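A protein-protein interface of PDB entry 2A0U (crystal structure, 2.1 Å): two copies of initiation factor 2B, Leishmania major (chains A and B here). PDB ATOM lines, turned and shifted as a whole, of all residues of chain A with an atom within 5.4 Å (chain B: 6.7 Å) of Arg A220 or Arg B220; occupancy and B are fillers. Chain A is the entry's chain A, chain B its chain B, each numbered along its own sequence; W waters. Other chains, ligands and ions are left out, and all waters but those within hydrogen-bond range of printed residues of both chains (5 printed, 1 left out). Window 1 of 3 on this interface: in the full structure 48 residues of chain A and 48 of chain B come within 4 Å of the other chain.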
ATOM      1  N   GLU A 218      -0.887   4.934   2.584  1.00  0.00           N
ATOM      2  CA  GLU A 218      -0.528   4.602   3.967  1.00  0.00           C
ATOM      3  C   GLU A 218       0.360   5.667   4.623  1.00  0.00           C
ATOM      4  O   GLU A 218       0.126   6.060   5.771  1.00  0.00           O
ATOM      5  CB  GLU A 218       0.158   3.230   4.014  1.00  0.00           C
ATOM      6  CG  GLU A 218       0.705   2.841   5.382  1.00  0.00           C
ATOM      7  CD  GLU A 218       1.116   1.385   5.471  1.00  0.00           C
ATOM      8  OE1 GLU A 218       1.585   0.817   4.457  1.00  0.00           O
ATOM      9  OE2 GLU A 218       0.977   0.810   6.570  1.00  0.00           O
ATOM     10  N   THR A 219       1.371   6.113   3.875  1.00  0.00           N
ATOM     11  CA  THR A 219       2.308   7.168   4.285  1.00  0.00           C
ATOM     12  C   THR A 219       3.279   6.728   5.392  1.00  0.00           C
ATOM     13  O   THR A 219       3.257   7.247   6.510  1.00  0.00           O
ATOM     14  CB  THR A 219       1.593   8.502   4.639  1.00  0.00           C
ATOM     15  OG1 THR A 219       0.590   8.785   3.658  1.00  0.00           O
ATOM     16  CG2 THR A 219       2.587   9.650   4.665  1.00  0.00           C
ATOM     17  N   ARG A 220       4.131   5.763   5.053  1.00  0.00           N
ATOM     18  CA  ARG A 220       5.217   5.321   5.921  1.00  0.00           C
ATOM     19  C   ARG A 220       6.232   6.453   6.142  1.00  0.00           C
ATOM     20  O   ARG A 220       6.363   7.336   5.288  1.00  0.00           O
ATOM     21  CB  ARG A 220       5.916   4.103   5.300  1.00  0.00           C
ATOM     22  CG  ARG A 220       5.095   2.810   5.296  1.00  0.00           C
ATOM     23  CD  ARG A 220       4.966   2.216   6.695  1.00  0.00           C
ATOM     24  NE  ARG A 220       6.253   1.781   7.235  1.00  0.00           N
ATOM     25  CZ  ARG A 220       6.564   1.757   8.527  1.00  0.00           C
ATOM     26  NH1 ARG A 220       7.765   1.342   8.906  1.00  0.00           N
ATOM     27  NH2 ARG A 220       5.686   2.153   9.444  1.00  0.00           N
ATOM     28  N   PRO A 221       6.961   6.432   7.280  1.00  0.00           N
ATOM     29  CA  PRO A 221       6.913   5.448   8.367  1.00  0.00           C
ATOM     30  C   PRO A 221       5.957   5.789   9.520  1.00  0.00           C
ATOM     31  O   PRO A 221       5.685   4.930  10.358  1.00  0.00           O
ATOM     32  CB  PRO A 221       8.354   5.440   8.876  1.00  0.00           C
ATOM     33  CG  PRO A 221       8.863   6.832   8.602  1.00  0.00           C
ATOM     34  CD  PRO A 221       7.987   7.461   7.536  1.00  0.00           C
ATOM     35  N   TRP A 222       5.463   7.024   9.559  1.00  0.00           N
ATOM     36  CA  TRP A 222       4.628   7.491  10.664  1.00  0.00           C
ATOM     37  C   TRP A 222       3.160   7.095  10.496  1.00  0.00           C
ATOM     38  O   TRP A 222       2.400   7.103  11.465  1.00  0.00           O
ATOM     39  CB  TRP A 222       4.771   9.008  10.834  1.00  0.00           C
ATOM     40  CG  TRP A 222       4.571   9.486  12.243  1.00  0.00           C
ATOM     41  CD1 TRP A 222       5.478   9.431  13.264  1.00  0.00           C
ATOM     42  CD2 TRP A 222       3.394  10.101  12.787  1.00  0.00           C
ATOM     43  NE1 TRP A 222       4.937   9.968  14.410  1.00  0.00           N
ATOM     44  CE2 TRP A 222       3.659  10.386  14.144  1.00  0.00           C
ATOM     45  CE3 TRP A 222       2.137  10.430  12.260  1.00  0.00           C
ATOM     46  CZ2 TRP A 222       2.717  10.992  14.982  1.00  0.00           C
ATOM     47  CZ3 TRP A 222       1.199  11.034  13.095  1.00  0.00           C
ATOM     48  CH2 TRP A 222       1.497  11.308  14.441  1.00  0.00           C
ATOM     49  N   ASN A 223       2.776   6.752   9.263  1.00  0.00           N
ATOM     50  CA  ASN A 223       1.430   6.256   8.930  1.00  0.00           C
ATOM     51  C   ASN A 223       0.292   7.263   9.136  1.00  0.00           C
ATOM     52  O   ASN A 223      -0.775   6.908   9.643  1.00  0.00           O
ATOM     53  CB  ASN A 223       1.125   4.930   9.653  1.00  0.00           C
ATOM     54  CG  ASN A 223       2.018   3.786   9.197  1.00  0.00           C
ATOM     55  OD1 ASN A 223       3.018   3.992   8.514  1.00  0.00           O
ATOM     56  ND2 ASN A 223       1.657   2.569   9.581  1.00  0.00           N
ATOM     57  N   CYS A 244      -1.107   0.816  -0.027  1.00  0.00           N
ATOM     58  CA  CYS A 244       0.308   0.966   0.299  1.00  0.00           C
ATOM     59  C   CYS A 244       0.923   1.990  -0.647  1.00  0.00           C
ATOM     60  O   CYS A 244       0.487   2.121  -1.793  1.00  0.00           O
ATOM     61  CB  CYS A 244       1.048  -0.369   0.179  1.00  0.00           C
ATOM     62  SG  CYS A 244       0.595  -1.590   1.426  1.00  0.00           S
ATOM     63  N   ASP A 245       1.936   2.705  -0.162  1.00  0.00           N
ATOM     64  CA  ASP A 245       2.582   3.774  -0.928  1.00  0.00           C
ATOM     65  C   ASP A 245       3.078   3.319  -2.304  1.00  0.00           C
ATOM     66  O   ASP A 245       2.944   4.051  -3.287  1.00  0.00           O
ATOM     67  CB  ASP A 245       3.730   4.391  -0.123  1.00  0.00           C
ATOM     68  CG  ASP A 245       3.276   4.938   1.222  1.00  0.00           C
ATOM     69  OD1 ASP A 245       2.220   5.603   1.277  1.00  0.00           O
ATOM     70  OD2 ASP A 245       3.983   4.707   2.226  1.00  0.00           O
ATOM     71  N   LYS A 276       5.235  15.906   2.829  1.00  0.00           N
ATOM     72  CA  LYS A 276       5.570  14.595   3.382  1.00  0.00           C
ATOM     73  C   LYS A 276       6.270  13.701   2.360  1.00  0.00           C
ATOM     74  O   LYS A 276       5.904  13.676   1.181  1.00  0.00           O
ATOM     75  CB  LYS A 276       4.319  13.899   3.932  1.00  0.00           C
ATOM     76  CG  LYS A 276       4.603  12.704   4.847  1.00  0.00           C
ATOM     77  CD  LYS A 276       5.131  13.131   6.216  1.00  0.00           C
ATOM     78  CE  LYS A 276       5.764  11.953   6.943  1.00  0.00           C
ATOM     79  NZ  LYS A 276       6.214  12.289   8.325  1.00  0.00           N
ATOM     80  N   ILE A 277       7.284  12.981   2.832  1.00  0.00           N
ATOM     81  CA  ILE A 277       8.040  12.040   2.014  1.00  0.00           C
ATOM     82  C   ILE A 277       7.086  11.111   1.247  1.00  0.00           C
ATOM     83  O   ILE A 277       6.117  10.590   1.814  1.00  0.00           O
ATOM     84  CB  ILE A 277       9.078  11.244   2.875  1.00  0.00           C
ATOM     85  CG1 ILE A 277      10.054  10.451   1.992  1.00  0.00           C
ATOM     86  CG2 ILE A 277       8.393  10.346   3.912  1.00  0.00           C
ATOM     87  CD1 ILE A 277      11.130  11.301   1.319  1.00  0.00           C
ATOM     88  N   GLU A 321      11.652   5.111  13.893  1.00  0.00           N
ATOM     89  CA  GLU A 321      10.364   5.262  13.211  1.00  0.00           C
ATOM     90  C   GLU A 321      10.162   4.168  12.161  1.00  0.00           C
ATOM     91  O   GLU A 321       9.033   3.754  11.893  1.00  0.00           O
ATOM     92  CB  GLU A 321      10.246   6.641  12.559  1.00  0.00           C
ATOM     93  CG  GLU A 321      10.147   7.794  13.549  1.00  0.00           C
ATOM     94  CD  GLU A 321       9.802   9.122  12.890  1.00  0.00           C
ATOM     95  OE1 GLU A 321       9.873   9.224  11.644  1.00  0.00           O
ATOM     96  OE2 GLU A 321       9.456  10.070  13.626  1.00  0.00           O
ATOM     97  N   ILE A 322      11.272   3.705  11.585  1.00  0.00           N
ATOM     98  CA  ILE A 322      11.266   2.643  10.582  1.00  0.00           C
ATOM     99  C   ILE A 322      11.601   1.274  11.193  1.00  0.00           C
ATOM    100  O   ILE A 322      10.976   0.267  10.852  1.00  0.00           O
ATOM    101  CB  ILE A 322      12.237   2.979   9.408  1.00  0.00           C
ATOM    102  CG1 ILE A 322      11.747   4.223   8.656  1.00  0.00           C
ATOM    103  CG2 ILE A 322      12.390   1.793   8.452  1.00  0.00           C
ATOM    104  CD1 ILE A 322      12.767   4.855   7.721  1.00  0.00           C
ATOM    105  N   CYS B 217      14.318  -0.960  -0.398  1.00  0.00           N
ATOM    106  CA  CYS B 217      12.967  -0.484  -0.120  1.00  0.00           C
ATOM    107  C   CYS B 217      12.319  -1.394   0.917  1.00  0.00           C
ATOM    108  O   CYS B 217      12.459  -2.618   0.842  1.00  0.00           O
ATOM    109  CB  CYS B 217      12.125  -0.472  -1.395  1.00  0.00           C
ATOM    110  SG  CYS B 217      12.622   0.752  -2.621  1.00  0.00           S
ATOM    111  N   GLU B 218      11.618  -0.789   1.876  1.00  0.00           N
ATOM    112  CA  GLU B 218      10.918  -1.523   2.937  1.00  0.00           C
ATOM    113  C   GLU B 218      10.032  -2.644   2.383  1.00  0.00           C
ATOM    114  O   GLU B 218      10.040  -3.761   2.904  1.00  0.00           O
ATOM    115  CB  GLU B 218      10.093  -0.556   3.797  1.00  0.00           C
ATOM    116  CG  GLU B 218       9.276  -1.225   4.902  1.00  0.00           C
ATOM    117  CD  GLU B 218       8.667  -0.232   5.875  1.00  0.00           C
ATOM    118  OE1 GLU B 218       8.042   0.755   5.425  1.00  0.00           O
ATOM    119  OE2 GLU B 218       8.809  -0.446   7.097  1.00  0.00           O
ATOM    120  N   THR B 219       9.287  -2.322   1.324  1.00  0.00           N
ATOM    121  CA  THR B 219       8.396  -3.253   0.617  1.00  0.00           C
ATOM    122  C   THR B 219       7.154  -3.648   1.428  1.00  0.00           C
ATOM    123  O   THR B 219       6.976  -4.814   1.794  1.00  0.00           O
ATOM    124  CB  THR B 219       9.137  -4.512   0.074  1.00  0.00           C
ATOM    125  OG1 THR B 219      10.449  -4.152  -0.384  1.00  0.00           O
ATOM    126  CG2 THR B 219       8.361  -5.122  -1.075  1.00  0.00           C
ATOM    127  N   ARG B 220       6.296  -2.663   1.688  1.00  0.00           N
ATOM    128  CA  ARG B 220       4.989  -2.896   2.311  1.00  0.00           C
ATOM    129  C   ARG B 220       4.083  -3.738   1.401  1.00  0.00           C
ATOM    130  O   ARG B 220       4.252  -3.719   0.176  1.00  0.00           O
ATOM    131  CB  ARG B 220       4.309  -1.561   2.643  1.00  0.00           C
ATOM    132  CG  ARG B 220       4.852  -0.849   3.889  1.00  0.00           C
ATOM    133  CD  ARG B 220       4.416  -1.542   5.178  1.00  0.00           C
ATOM    134  NE  ARG B 220       2.993  -1.354   5.463  1.00  0.00           N
ATOM    135  CZ  ARG B 220       2.248  -2.192   6.179  1.00  0.00           C
ATOM    136  NH1 ARG B 220       0.966  -1.926   6.383  1.00  0.00           N
ATOM    137  NH2 ARG B 220       2.775  -3.300   6.688  1.00  0.00           N
ATOM    138  N   PRO B 221       3.112  -4.473   1.987  1.00  0.00           N
ATOM    139  CA  PRO B 221       2.785  -4.582   3.411  1.00  0.00           C
ATOM    140  C   PRO B 221       3.496  -5.713   4.167  1.00  0.00           C
ATOM    141  O   PRO B 221       3.480  -5.720   5.397  1.00  0.00           O
ATOM    142  CB  PRO B 221       1.280  -4.848   3.388  1.00  0.00           C
ATOM    143  CG  PRO B 221       1.050  -5.596   2.102  1.00  0.00           C
ATOM    144  CD  PRO B 221       2.190  -5.278   1.161  1.00  0.00           C
ATOM    145  N   TRP B 222       4.101  -6.651   3.443  1.00  0.00           N
ATOM    146  CA  TRP B 222       4.707  -7.837   4.055  1.00  0.00           C
ATOM    147  C   TRP B 222       6.122  -7.575   4.573  1.00  0.00           C
ATOM    148  O   TRP B 222       6.643  -8.341   5.388  1.00  0.00           O
ATOM    149  CB  TRP B 222       4.707  -9.002   3.060  1.00  0.00           C
ATOM    150  CG  TRP B 222       4.627 -10.361   3.703  1.00  0.00           C
ATOM    151  CD1 TRP B 222       3.511 -10.960   4.217  1.00  0.00           C
ATOM    152  CD2 TRP B 222       5.701 -11.297   3.880  1.00  0.00           C
ATOM    153  NE1 TRP B 222       3.824 -12.204   4.710  1.00  0.00           N
ATOM    154  CE2 TRP B 222       5.161 -12.437   4.515  1.00  0.00           C
ATOM    155  CE3 TRP B 222       7.068 -11.280   3.570  1.00  0.00           C
ATOM    156  CZ2 TRP B 222       5.940 -13.555   4.843  1.00  0.00           C
ATOM    157  CZ3 TRP B 222       7.843 -12.391   3.897  1.00  0.00           C
ATOM    158  CH2 TRP B 222       7.274 -13.513   4.529  1.00  0.00           C
ATOM    159  N   ASN B 223       6.731  -6.490   4.090  1.00  0.00           N
ATOM    160  CA  ASN B 223       8.061  -6.032   4.525  1.00  0.00           C
ATOM    161  C   ASN B 223       9.222  -6.988   4.221  1.00  0.00           C
ATOM    162  O   ASN B 223      10.086  -7.218   5.069  1.00  0.00           O
ATOM    163  CB  ASN B 223       8.056  -5.613   6.005  1.00  0.00           C
ATOM    164  CG  ASN B 223       7.218  -4.375   6.258  1.00  0.00           C
ATOM    165  OD1 ASN B 223       6.747  -3.727   5.326  1.00  0.00           O
ATOM    166  ND2 ASN B 223       7.030  -4.040   7.527  1.00  0.00           N
ATOM    167  N   GLN B 224       9.237  -7.524   3.000  1.00  0.00           N
ATOM    168  CA  GLN B 224      10.332  -8.381   2.534  1.00  0.00           C
ATOM    169  C   GLN B 224      11.678  -7.658   2.584  1.00  0.00           C
ATOM    170  O   GLN B 224      12.707  -8.264   2.893  1.00  0.00           O
ATOM    171  CB  GLN B 224      10.075  -8.869   1.103  1.00  0.00           C
ATOM    172  CG  GLN B 224       9.029  -9.973   0.970  1.00  0.00           C
ATOM    173  CD  GLN B 224       7.620  -9.451   0.711  1.00  0.00           C
ATOM    174  OE1 GLN B 224       7.311  -8.281   0.956  1.00  0.00           O
ATOM    175  NE2 GLN B 224       6.755 -10.327   0.209  1.00  0.00           N
ATOM    176  N   GLY B 225      11.659  -6.363   2.272  1.00  0.00           N
ATOM    177  CA  GLY B 225      12.864  -5.540   2.272  1.00  0.00           C
ATOM    178  C   GLY B 225      13.401  -5.262   3.661  1.00  0.00           C
ATOM    179  O   GLY B 225      14.568  -5.542   3.946  1.00  0.00           O
ATOM    180  N   CYS B 244      11.986   3.888   3.141  1.00  0.00           N
ATOM    181  CA  CYS B 244      10.566   3.666   2.904  1.00  0.00           C
ATOM    182  C   CYS B 244      10.302   3.714   1.406  1.00  0.00           C
ATOM    183  O   CYS B 244      11.011   4.401   0.667  1.00  0.00           O
ATOM    184  CB  CYS B 244       9.726   4.703   3.644  1.00  0.00           C
ATOM    185  SG  CYS B 244       9.833   4.534   5.429  1.00  0.00           S
ATOM    186  N   ASP B 245       9.289   2.972   0.968  1.00  0.00           N
ATOM    187  CA  ASP B 245       8.962   2.843  -0.454  1.00  0.00           C
ATOM    188  C   ASP B 245       8.762   4.190  -1.156  1.00  0.00           C
ATOM    189  O   ASP B 245       9.226   4.381  -2.282  1.00  0.00           O
ATOM    190  CB  ASP B 245       7.734   1.942  -0.638  1.00  0.00           C
ATOM    191  CG  ASP B 245       7.932   0.554  -0.045  1.00  0.00           C
ATOM    192  OD1 ASP B 245       9.045  -0.002  -0.180  1.00  0.00           O
ATOM    193  OD2 ASP B 245       6.976   0.017   0.555  1.00  0.00           O
ATOM    194  N   GLY B 246       8.097   5.122  -0.473  1.00  0.00           N
ATOM    195  CA  GLY B 246       7.814   6.451  -1.020  1.00  0.00           C
ATOM    196  C   GLY B 246       9.023   7.363  -1.183  1.00  0.00           C
ATOM    197  O   GLY B 246       8.955   8.364  -1.897  1.00  0.00           O
ATOM    198  N   LYS B 276       6.895  -8.010  -7.293  1.00  0.00           N
ATOM    199  CA  LYS B 276       6.289  -7.476  -6.074  1.00  0.00           C
ATOM    200  C   LYS B 276       5.768  -6.051  -6.262  1.00  0.00           C
ATOM    201  O   LYS B 276       6.418  -5.210  -6.887  1.00  0.00           O
ATOM    202  CB  LYS B 276       7.276  -7.541  -4.900  1.00  0.00           C
ATOM    203  CG  LYS B 276       6.649  -7.322  -3.517  1.00  0.00           C
ATOM    204  CD  LYS B 276       5.829  -8.525  -3.042  1.00  0.00           C
ATOM    205  CE  LYS B 276       4.935  -8.143  -1.865  1.00  0.00           C
ATOM    206  NZ  LYS B 276       4.177  -9.299  -1.295  1.00  0.00           N
ATOM    207  N   ILE B 277       4.575  -5.808  -5.719  1.00  0.00           N
ATOM    208  CA  ILE B 277       3.933  -4.496  -5.754  1.00  0.00           C
ATOM    209  C   ILE B 277       4.924  -3.384  -5.370  1.00  0.00           C
ATOM    210  O   ILE B 277       5.670  -3.506  -4.391  1.00  0.00           O
ATOM    211  CB  ILE B 277       2.637  -4.472  -4.866  1.00  0.00           C
ATOM    212  CG1 ILE B 277       1.848  -3.165  -5.036  1.00  0.00           C
ATOM    213  CG2 ILE B 277       2.956  -4.749  -3.387  1.00  0.00           C
ATOM    214  CD1 ILE B 277       1.082  -3.053  -6.349  1.00  0.00           C
ATOM    215  N   GLY B 278       4.948  -2.324  -6.176  1.00  0.00           N
ATOM    216  CA  GLY B 278       5.900  -1.230  -5.995  1.00  0.00           C
ATOM    217  C   GLY B 278       7.016  -1.212  -7.027  1.00  0.00           C
ATOM    218  O   GLY B 278       7.671  -0.184  -7.221  1.00  0.00           O
ATOM    219  N   GLU B 321      -3.123  -7.862   6.119  1.00  0.00           N
ATOM    220  CA  GLU B 321      -1.702  -7.601   5.875  1.00  0.00           C
ATOM    221  C   GLU B 321      -1.382  -6.111   6.016  1.00  0.00           C
ATOM    222  O   GLU B 321      -0.276  -5.741   6.406  1.00  0.00           O
ATOM    223  CB  GLU B 321      -1.282  -8.097   4.484  1.00  0.00           C
ATOM    224  CG  GLU B 321      -1.197  -9.617   4.345  1.00  0.00           C
ATOM    225  CD  GLU B 321      -0.566 -10.072   3.031  1.00  0.00           C
ATOM    226  OE1 GLU B 321      -0.390  -9.242   2.110  1.00  0.00           O
ATOM    227  OE2 GLU B 321      -0.245 -11.274   2.917  1.00  0.00           O
ATOM    228  N   ILE B 322      -2.363  -5.269   5.697  1.00  0.00           N
ATOM    229  CA  ILE B 322      -2.230  -3.816   5.792  1.00  0.00           C
ATOM    230  C   ILE B 322      -2.856  -3.266   7.083  1.00  0.00           C
ATOM    231  O   ILE B 322      -2.292  -2.370   7.716  1.00  0.00           O
ATOM    232  CB  ILE B 322      -2.835  -3.108   4.540  1.00  0.00           C
ATOM    233  CG1 ILE B 322      -2.194  -3.657   3.255  1.00  0.00           C
ATOM    234  CG2 ILE B 322      -2.666  -1.586   4.628  1.00  0.00           C
ATOM    235  CD1 ILE B 322      -2.779  -3.122   1.962  1.00  0.00           C
ATOM    236  N   THR B 323      -4.006  -3.816   7.475  1.00  0.00           N
ATOM    237  CA  THR B 323      -4.797  -3.264   8.583  1.00  0.00           C
ATOM    238  C   THR B 323      -4.392  -3.748   9.980  1.00  0.00           C
ATOM    239  O   THR B 323      -4.746  -3.118  10.981  1.00  0.00           O
ATOM    240  CB  THR B 323      -6.314  -3.500   8.385  1.00  0.00           C
ATOM    241  OG1 THR B 323      -6.569  -4.898   8.203  1.00  0.00           O
ATOM    242  CG2 THR B 323      -6.827  -2.730   7.178  1.00  0.00           C
ATOM    243  N   THR B 324      -3.662  -4.861  10.048  1.00  0.00           N
ATOM    244  CA  THR B 324      -3.261  -5.435  11.335  1.00  0.00           C
ATOM    245  C   THR B 324      -1.748  -5.576  11.488  1.00  0.00           C
ATOM    246  O   THR B 324      -1.031  -5.779  10.506  1.00  0.00           O
ATOM    247  CB  THR B 324      -3.914  -6.823  11.599  1.00  0.00           C
ATOM    248  OG1 THR B 324      -3.429  -7.782  10.652  1.00  0.00           O
ATOM    249  CG2 THR B 324      -5.433  -6.746  11.517  1.00  0.00           C
ATOM    250  N   LEU B 326       1.477  -7.452  12.122  1.00  0.00           N
ATOM    251  CA  LEU B 326       1.751  -8.794  11.600  1.00  0.00           C
ATOM    252  C   LEU B 326       2.033  -9.862  12.653  1.00  0.00           C
ATOM    253  O   LEU B 326       3.153 -10.041  13.134  1.00  0.00           O
ATOM    254  CB  LEU B 326       2.848  -8.765  10.526  1.00  0.00           C
ATOM    255  CG  LEU B 326       2.567  -9.441   9.172  1.00  0.00           C
ATOM    256  CD1 LEU B 326       3.873  -9.939   8.546  1.00  0.00           C
ATOM    257  CD2 LEU B 326       1.528 -10.577   9.236  1.00  0.00           C
ATOM    258  N   VAL B 332      -4.373  -1.768  13.448  1.00  0.00           N
ATOM    259  CA  VAL B 332      -3.734  -0.453  13.558  1.00  0.00           C
ATOM    260  C   VAL B 332      -4.433   0.573  12.656  1.00  0.00           C
ATOM    261  O   VAL B 332      -4.024   1.734  12.574  1.00  0.00           O
ATOM    262  CB  VAL B 332      -2.218  -0.527  13.236  1.00  0.00           C
ATOM    263  CG1 VAL B 332      -1.459  -1.159  14.396  1.00  0.00           C
ATOM    264  CG2 VAL B 332      -1.966  -1.296  11.934  1.00  0.00           C
ATOM    265  N   ASN B 343      -5.261  -4.546  -1.818  1.00  0.00           N
ATOM    266  CA  ASN B 343      -4.000  -5.232  -1.527  1.00  0.00           C
ATOM    267  C   ASN B 343      -3.516  -6.183  -2.634  1.00  0.00           C
ATOM    268  O   ASN B 343      -3.461  -7.399  -2.431  1.00  0.00           O
ATOM    269  CB  ASN B 343      -4.073  -5.953  -0.171  1.00  0.00           C
ATOM    270  CG  ASN B 343      -2.723  -6.507   0.278  1.00  0.00           C
ATOM    271  OD1 ASN B 343      -1.673  -5.908   0.033  1.00  0.00           O
ATOM    272  ND2 ASN B 343      -2.752  -7.658   0.942  1.00  0.00           N
ATOM    273  N   PRO B 344      -3.167  -5.634  -3.814  1.00  0.00           N
ATOM    274  CA  PRO B 344      -2.464  -6.485  -4.767  1.00  0.00           C
ATOM    275  C   PRO B 344      -1.004  -6.626  -4.335  1.00  0.00           C
ATOM    276  O   PRO B 344      -0.387  -5.643  -3.915  1.00  0.00           O
ATOM    277  CB  PRO B 344      -2.581  -5.714  -6.082  1.00  0.00           C
ATOM    278  CG  PRO B 344      -2.681  -4.285  -5.672  1.00  0.00           C
ATOM    279  CD  PRO B 344      -3.377  -4.269  -4.338  1.00  0.00           C
HETATM  280  O   HOH W   1       6.600   4.200   1.878  1.00  0.00           O
HETATM  281  O   HOH W   2      10.234  -1.772   9.108  1.00  0.00           O
HETATM  282  O   HOH W   3      -1.363   1.806  10.591  1.00  0.00           O
HETATM  283  O   HOH W   4       4.391   0.612  -0.160  1.00  0.00           O
HETATM  284  O   HOH W   5      -1.208   0.252   8.182  1.00  0.00           O
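OE1 of Glu B218 lies within salt-bridge range of NE of Arg A220 (2.7 Å).
The side-chain carboxylate (OE2) of Glu A218 lies within salt-bridge range of the guanidinium group (NH1) of Arg B220, at 2.7 Å.
The backbone NH (N) of Arg B220 lies within hydrogen-bond range of the side-chain carboxylate (OD2) of Asp B245, at 3.0 Å.
The side-chain amide oxygen (OD1) of Asn A223 lies close to the backbone carbonyl oxygen (O) of Pro A221, 3.4 Å away.
NH2 of Arg A220 lies close to OD1 of Asn A223, at 3.4 Å.
N of Glu B218 is in hydrogen-bond range of OD1 of Asp B245, 3.4 Å away.
The backbone carbonyl oxygen (O) of Glu B218 sits at hydrogen-bond distance from the backbone NH (N) of Gly B225 (3.1 Å).
OD1 of Asp A245 sits at hydrogen-bond distance from N of Glu A218 (3.4 Å).
Arg B220 touches Arg A220.
Arg A220 touches Cys B244 (CB to SG, 3.9 Å).
Pro A221 touches Cys B244 (CB to SG, 3.9 Å).
Arg B220 touches Cys A244.
Cys A244 touches Pro B221 (SG to CB, 3.9 Å).
Ile B322 touches Cys A244 (CD1 to SG, 3.7 Å).
Ile A322 touches Cys B244 (CD1 to SG, 3.7 Å).
Of the printed residues of chain B, Arg A220 touches Glu B218 (2.7 Å), Arg B220 (3.9 Å) and Cys B244 (3.9 Å).
Of the printed residues of chain B, Ile A322 touches Cys B244 (3.7 Å).
Of chain A, only Glu A218 (2.7 Å), Arg A220 (3.9 Å) and Cys A244 (3.9 Å) come within 4 Å of Arg B220.
Of the printed residues of chain A, Cys B244 touches Arg A220, Pro A221 and Ile A322.
Ile B277 touches none of the printed residues of chain A.
The nearest printed residue of chain A that does not touch Arg B220 is Asn A223 (5.6 Å).
Of the 12 printed residues of chain A, 5 touch a printed residue of chain B.
Printed residues of chain A that touch a printed residue of chain B: Glu A218, Arg A220, Pro A221, Cys A244 and Ile A322.
Hydrophobic or aromatic side chains of chain A that line the printed part of chain B: Pro A221 and Ile A322.
Among the printed residues, 9 pairs touch across the chains.
Glu A218 touches Arg B220, and with the chains exchanged Arg A220 touches Glu B218.
Arg A220 touches its own counterpart, Arg B220.
Pro A221 touches Cys B244, and with the chains exchanged Cys A244 touches Pro B221.
Cys A244 touches Ile B322, and with the chains exchanged Ile A322 touches Cys B244.
12 positions are printed for both chains.
Water W1 lies within hydrogen-bond range of the side-chain carboxylate (OD2) of Asp A245 (2.7 Å), the backbone NH (N) of Gly B246 (2.9 Å) and the backbone NH (N) of Asp B245 (3.1 Å).
Water W4 bridges OD2 of Asp B245 (2.7 Å) and N of Asp A245 (3.2 Å).
Water W5 lies within hydrogen-bond range of the side-chain carboxylate (OE2) of Glu A218 (2.8 Å) and the backbone carbonyl oxygen (O) of Ile B322 (2.9 Å).
Water W2 lies within hydrogen-bond range of O of Ile A322 (2.8 Å) and OE2 of Glu B218 (2.8 Å).
Water W3 lies within hydrogen-bond range of ND2 of Asn A223 (3.3 Å) and O of Val B332 (3.3 Å).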
